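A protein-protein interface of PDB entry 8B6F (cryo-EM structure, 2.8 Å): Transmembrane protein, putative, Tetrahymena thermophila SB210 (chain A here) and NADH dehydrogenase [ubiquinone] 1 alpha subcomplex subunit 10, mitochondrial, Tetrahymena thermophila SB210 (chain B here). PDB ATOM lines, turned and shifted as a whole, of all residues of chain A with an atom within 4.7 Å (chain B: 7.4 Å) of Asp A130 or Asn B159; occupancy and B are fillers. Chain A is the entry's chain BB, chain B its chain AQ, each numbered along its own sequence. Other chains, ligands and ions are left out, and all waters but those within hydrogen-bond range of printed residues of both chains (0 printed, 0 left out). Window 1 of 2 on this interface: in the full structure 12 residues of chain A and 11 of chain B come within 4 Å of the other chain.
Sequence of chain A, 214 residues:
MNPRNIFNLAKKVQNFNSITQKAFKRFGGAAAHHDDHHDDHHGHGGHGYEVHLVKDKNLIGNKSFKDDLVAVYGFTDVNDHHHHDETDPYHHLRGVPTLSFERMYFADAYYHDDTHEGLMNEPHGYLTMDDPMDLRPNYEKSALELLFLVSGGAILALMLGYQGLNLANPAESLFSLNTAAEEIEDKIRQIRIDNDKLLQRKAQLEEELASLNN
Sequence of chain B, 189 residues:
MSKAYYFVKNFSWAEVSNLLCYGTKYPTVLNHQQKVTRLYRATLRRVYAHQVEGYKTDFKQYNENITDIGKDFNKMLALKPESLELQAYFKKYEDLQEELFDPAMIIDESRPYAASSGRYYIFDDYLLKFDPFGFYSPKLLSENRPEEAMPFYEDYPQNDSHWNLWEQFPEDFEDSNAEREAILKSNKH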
ATOM      1  N   THR A 128      -4.220   0.400  19.876  1.00  0.00           N
ATOM      2  CA  THR A 128      -3.586  -0.872  19.567  1.00  0.00           C
ATOM      3  C   THR A 128      -3.924  -1.263  18.135  1.00  0.00           C
ATOM      4  O   THR A 128      -4.631  -0.549  17.421  1.00  0.00           O
ATOM      5  CB  THR A 128      -4.037  -1.972  20.530  1.00  0.00           C
ATOM      6  OG1 THR A 128      -5.459  -2.099  20.458  1.00  0.00           O
ATOM      7  CG2 THR A 128      -3.633  -1.633  21.958  1.00  0.00           C
ATOM      8  N   MET A 129      -3.411  -2.418  17.717  1.00  0.00           N
ATOM      9  CA  MET A 129      -3.656  -2.915  16.371  1.00  0.00           C
ATOM     10  C   MET A 129      -4.978  -3.660  16.246  1.00  0.00           C
ATOM     11  O   MET A 129      -5.348  -4.046  15.133  1.00  0.00           O
ATOM     12  CB  MET A 129      -2.506  -3.829  15.944  1.00  0.00           C
ATOM     13  CG  MET A 129      -2.548  -4.230  14.484  1.00  0.00           C
ATOM     14  SD  MET A 129      -0.964  -4.848  13.892  1.00  0.00           S
ATOM     15  CE  MET A 129      -0.701  -6.223  15.005  1.00  0.00           C
ATOM     16  N   ASP A 130      -5.698  -3.869  17.346  1.00  0.00           N
ATOM     17  CA  ASP A 130      -6.980  -4.556  17.279  1.00  0.00           C
ATOM     18  C   ASP A 130      -8.020  -3.694  16.574  1.00  0.00           C
ATOM     19  O   ASP A 130      -8.117  -2.487  16.811  1.00  0.00           O
ATOM     20  CB  ASP A 130      -7.469  -4.914  18.682  1.00  0.00           C
ATOM     21  CG  ASP A 130      -6.628  -5.991  19.332  1.00  0.00           C
ATOM     22  OD1 ASP A 130      -5.523  -6.268  18.825  1.00  0.00           O
ATOM     23  OD2 ASP A 130      -7.079  -6.572  20.341  1.00  0.00           O
ATOM     24  N   ASP A 131      -8.808  -4.326  15.714  1.00  0.00           N
ATOM     25  CA  ASP A 131      -9.838  -3.606  14.975  1.00  0.00           C
ATOM     26  C   ASP A 131     -11.005  -3.278  15.902  1.00  0.00           C
ATOM     27  O   ASP A 131     -11.555  -4.183  16.537  1.00  0.00           O
ATOM     28  CB  ASP A 131     -10.315  -4.448  13.794  1.00  0.00           C
ATOM     29  CG  ASP A 131     -11.251  -3.691  12.871  1.00  0.00           C
ATOM     30  OD1 ASP A 131     -11.920  -2.744  13.334  1.00  0.00           O
ATOM     31  OD2 ASP A 131     -11.325  -4.049  11.678  1.00  0.00           O
ATOM     32  N   PRO A 132     -11.412  -2.008  16.011  1.00  0.00           N
ATOM     33  CA  PRO A 132     -12.560  -1.697  16.878  1.00  0.00           C
ATOM     34  C   PRO A 132     -13.819  -2.457  16.506  1.00  0.00           C
ATOM     35  O   PRO A 132     -14.587  -2.847  17.393  1.00  0.00           O
ATOM     36  CB  PRO A 132     -12.739  -0.184  16.690  1.00  0.00           C
ATOM     37  CG  PRO A 132     -11.415   0.306  16.253  1.00  0.00           C
ATOM     38  CD  PRO A 132     -10.817  -0.792  15.431  1.00  0.00           C
ATOM     39  N   ARG A 136     -14.593 -11.354  14.812  1.00  0.00           N
ATOM     40  CA  ARG A 136     -14.015 -12.584  15.336  1.00  0.00           C
ATOM     41  C   ARG A 136     -14.310 -12.709  16.830  1.00  0.00           C
ATOM     42  O   ARG A 136     -14.156 -11.739  17.574  1.00  0.00           O
ATOM     43  CB  ARG A 136     -12.506 -12.611  15.107  1.00  0.00           C
ATOM     44  CG  ARG A 136     -12.114 -12.727  13.651  1.00  0.00           C
ATOM     45  CD  ARG A 136     -10.621 -12.937  13.485  1.00  0.00           C
ATOM     46  NE  ARG A 136      -9.857 -11.756  13.863  1.00  0.00           N
ATOM     47  CZ  ARG A 136      -8.538 -11.653  13.761  1.00  0.00           C
ATOM     48  NH1 ARG A 136      -7.800 -12.648  13.300  1.00  0.00           N
ATOM     49  NH2 ARG A 136      -7.947 -10.520  14.126  1.00  0.00           N
ATOM     50  N   ASN A 138     -12.592 -13.392  19.255  1.00  0.00           N
ATOM     51  CA  ASN A 138     -11.233 -13.528  19.756  1.00  0.00           C
ATOM     52  C   ASN A 138     -11.205 -13.409  21.276  1.00  0.00           C
ATOM     53  O   ASN A 138     -11.918 -12.589  21.860  1.00  0.00           O
ATOM     54  CB  ASN A 138     -10.342 -12.465  19.122  1.00  0.00           C
ATOM     55  CG  ASN A 138      -8.890 -12.631  19.486  1.00  0.00           C
ATOM     56  OD1 ASN A 138      -8.478 -13.680  19.974  1.00  0.00           O
ATOM     57  ND2 ASN A 138      -8.100 -11.596  19.243  1.00  0.00           N
ATOM     58  N   GLU A 140      -7.948 -13.744  23.167  1.00  0.00           N
ATOM     59  CA  GLU A 140      -6.618 -13.539  23.729  1.00  0.00           C
ATOM     60  C   GLU A 140      -6.612 -12.373  24.710  1.00  0.00           C
ATOM     61  O   GLU A 140      -6.020 -12.468  25.791  1.00  0.00           O
ATOM     62  CB  GLU A 140      -5.602 -13.313  22.612  1.00  0.00           C
ATOM     63  CG  GLU A 140      -5.888 -12.099  21.751  1.00  0.00           C
ATOM     64  CD  GLU A 140      -4.988 -12.026  20.535  1.00  0.00           C
ATOM     65  OE1 GLU A 140      -4.343 -13.044  20.214  1.00  0.00           O
ATOM     66  OE2 GLU A 140      -4.922 -10.950  19.908  1.00  0.00           O
ATOM     67  N   PHE B 133      -8.822   0.567   9.594  1.00  0.00           N
ATOM     68  CA  PHE B 133     -10.131   0.665  10.215  1.00  0.00           C
ATOM     69  C   PHE B 133     -10.860   1.887   9.665  1.00  0.00           C
ATOM     70  O   PHE B 133     -10.258   2.786   9.076  1.00  0.00           O
ATOM     71  CB  PHE B 133      -9.994   0.740  11.736  1.00  0.00           C
ATOM     72  CG  PHE B 133      -8.977  -0.216  12.297  1.00  0.00           C
ATOM     73  CD1 PHE B 133      -8.799  -1.471  11.737  1.00  0.00           C
ATOM     74  CD2 PHE B 133      -8.186   0.146  13.373  1.00  0.00           C
ATOM     75  CE1 PHE B 133      -7.857  -2.346  12.247  1.00  0.00           C
ATOM     76  CE2 PHE B 133      -7.245  -0.723  13.885  1.00  0.00           C
ATOM     77  CZ  PHE B 133      -7.079  -1.971  13.323  1.00  0.00           C
ATOM     78  N   TYR B 156      -6.235  -9.310   4.113  1.00  0.00           N
ATOM     79  CA  TYR B 156      -5.618  -9.869   5.306  1.00  0.00           C
ATOM     80  C   TYR B 156      -5.777  -8.887   6.462  1.00  0.00           C
ATOM     81  O   TYR B 156      -5.418  -7.711   6.321  1.00  0.00           O
ATOM     82  CB  TYR B 156      -4.144 -10.165   5.060  1.00  0.00           C
ATOM     83  CG  TYR B 156      -3.890 -11.523   4.454  1.00  0.00           C
ATOM     84  CD1 TYR B 156      -3.752 -12.645   5.258  1.00  0.00           C
ATOM     85  CD2 TYR B 156      -3.786 -11.683   3.081  1.00  0.00           C
ATOM     86  CE1 TYR B 156      -3.519 -13.890   4.713  1.00  0.00           C
ATOM     87  CE2 TYR B 156      -3.553 -12.924   2.524  1.00  0.00           C
ATOM     88  CZ  TYR B 156      -3.420 -14.024   3.346  1.00  0.00           C
ATOM     89  OH  TYR B 156      -3.188 -15.263   2.800  1.00  0.00           O
ATOM     90  N   PRO B 157      -6.304  -9.316   7.606  1.00  0.00           N
ATOM     91  CA  PRO B 157      -6.487  -8.381   8.719  1.00  0.00           C
ATOM     92  C   PRO B 157      -5.158  -7.935   9.301  1.00  0.00           C
ATOM     93  O   PRO B 157      -4.141  -8.624   9.198  1.00  0.00           O
ATOM     94  CB  PRO B 157      -7.295  -9.194   9.736  1.00  0.00           C
ATOM     95  CG  PRO B 157      -6.932 -10.600   9.452  1.00  0.00           C
ATOM     96  CD  PRO B 157      -6.711 -10.685   7.970  1.00  0.00           C
ATOM     97  N   GLN B 158      -5.176  -6.751   9.916  1.00  0.00           N
ATOM     98  CA  GLN B 158      -3.977  -6.248  10.575  1.00  0.00           C
ATOM     99  C   GLN B 158      -3.545  -7.180  11.700  1.00  0.00           C
ATOM    100  O   GLN B 158      -2.362  -7.509  11.832  1.00  0.00           O
ATOM    101  CB  GLN B 158      -4.229  -4.837  11.108  1.00  0.00           C
ATOM    102  CG  GLN B 158      -4.525  -3.820  10.021  1.00  0.00           C
ATOM    103  CD  GLN B 158      -3.355  -3.620   9.081  1.00  0.00           C
ATOM    104  OE1 GLN B 158      -2.197  -3.701   9.489  1.00  0.00           O
ATOM    105  NE2 GLN B 158      -3.650  -3.362   7.814  1.00  0.00           N
ATOM    106  N   ASN B 159      -4.496  -7.624  12.514  1.00  0.00           N
ATOM    107  CA  ASN B 159      -4.240  -8.590  13.573  1.00  0.00           C
ATOM    108  C   ASN B 159      -4.699  -9.960  13.093  1.00  0.00           C
ATOM    109  O   ASN B 159      -5.884 -10.154  12.804  1.00  0.00           O
ATOM    110  CB  ASN B 159      -4.967  -8.193  14.856  1.00  0.00           C
ATOM    111  CG  ASN B 159      -4.615  -9.085  16.027  1.00  0.00           C
ATOM    112  OD1 ASN B 159      -3.559  -9.714  16.047  1.00  0.00           O
ATOM    113  ND2 ASN B 159      -5.501  -9.145  17.012  1.00  0.00           N
ATOM    114  N   ASP B 160      -3.764 -10.907  13.012  1.00  0.00           N
ATOM    115  CA  ASP B 160      -4.035 -12.235  12.478  1.00  0.00           C
ATOM    116  C   ASP B 160      -4.045 -13.301  13.570  1.00  0.00           C
ATOM    117  O   ASP B 160      -3.725 -14.463  13.312  1.00  0.00           O
ATOM    118  CB  ASP B 160      -3.012 -12.594  11.402  1.00  0.00           C
ATOM    119  CG  ASP B 160      -1.614 -12.745  11.959  1.00  0.00           C
ATOM    120  OD1 ASP B 160      -1.324 -12.132  13.006  1.00  0.00           O
ATOM    121  OD2 ASP B 160      -0.807 -13.478  11.350  1.00  0.00           O
ATOM    122  N   SER B 161      -4.403 -12.920  14.792  1.00  0.00           N
ATOM    123  CA  SER B 161      -4.476 -13.885  15.878  1.00  0.00           C
ATOM    124  C   SER B 161      -5.542 -14.931  15.580  1.00  0.00           C
ATOM    125  O   SER B 161      -6.647 -14.608  15.137  1.00  0.00           O
ATOM    126  CB  SER B 161      -4.781 -13.179  17.197  1.00  0.00           C
ATOM    127  OG  SER B 161      -6.008 -12.478  17.125  1.00  0.00           O
ATOM    128  N   HIS B 162      -5.200 -16.195  15.824  1.00  0.00           N
ATOM    129  CA  HIS B 162      -6.100 -17.312  15.584  1.00  0.00           C
ATOM    130  C   HIS B 162      -6.793 -17.788  16.853  1.00  0.00           C
ATOM    131  O   HIS B 162      -7.409 -18.858  16.847  1.00  0.00           O
ATOM    132  CB  HIS B 162      -5.340 -18.474  14.942  1.00  0.00           C
ATOM    133  CG  HIS B 162      -4.803 -18.161  13.580  1.00  0.00           C
ATOM    134  ND1 HIS B 162      -5.574 -18.243  12.441  1.00  0.00           N
ATOM    135  CD2 HIS B 162      -3.574 -17.765  13.176  1.00  0.00           C
ATOM    136  CE1 HIS B 162      -4.842 -17.911  11.393  1.00  0.00           C
ATOM    137  NE2 HIS B 162      -3.625 -17.617  11.811  1.00  0.00           N
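O of Met A129 touches CZ of Phe B133 (3.3 Å). Asp A130 touches Phe B133 (O to CE2, 3.5 Å). Asp A131 touches Phe B133. Phe B133 touches Pro A132 (CD2 to CD, 3.5 Å). NH1 of Arg A136 touches C of Asp B160 (3.8 Å).
NH1 of Arg A136 sits at hydrogen-bond distance from O of Ser B161, at 2.9 Å. OE2 of Glu A140 is in hydrogen-bond range of OG of Ser B161 (3.4 Å). The side-chain amide nitrogen of Asn B159 is in hydrogen-bond range of the side-chain carboxylate of Glu A140 (3.5 Å). ND2 of Asn A138 sits at hydrogen-bond distance from OG of Ser B161 (3.1 Å). OD1 of Asp A130 lies within hydrogen-bond range of ND2 of Asn B159, 3.4 Å away. NH2 of Arg A136 sits at hydrogen-bond distance from O of Asn B159 (2.5 Å). The side-chain sulfur of Met A129 sits close to the backbone carbonyl oxygen of Gln B158, 3.6 Å away.
Of the 8 printed residues of chain B, 5 touch a printed residue of chain A. Hydrophobic or aromatic side chains of chain B within 4 Å of the printed part of chain A: Phe B133. Of the 8 printed residues of chain A, 7 touch a printed residue of chain B. Among the printed residues, no Asp or Glu carboxylate lies within 4 Å of a Lys or Arg side-chain nitrogen of the other chain.
The backbone carbonyl oxygen (O) of Asp B160 sits close to a ring nitrogen (NE2) of His B162. The side-chain amide oxygen (OD1) of Asn A138 lies within hydrogen-bond range of the backbone NH (N) of Glu A140. OG of Ser B161 sits at hydrogen-bond distance from ND2 of Asn B159 (3.4 Å).
Of the printed residues of chain B, Met A129 touches Phe B133 and Gln B158. Asp A130 touches just these residues of chain B: Phe B133 and Asn B159. Of the printed residues of chain B, Asp A131 touches Phe B133. Of the printed residues of chain B, Asn A138 touches Ser B161 (3.1 Å). Printed residues of chain A within 4 Å of Phe B133: Met A129 (3.3 Å), Asp A130 (3.5 Å), Asp A131 (3.5 Å) and Pro A132 (3.5 Å). Asn B159 touches just these residues of chain A: Asp A130 (3.4 Å), Arg A136 (2.5 Å) and Glu A140 (3.5 Å). The nearest printed residue of chain B that does not touch Asp A130 is Ser B161 (6.5 Å). The nearest printed residue of chain B that does not touch Glu A140 is His B162 (5.5 Å).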
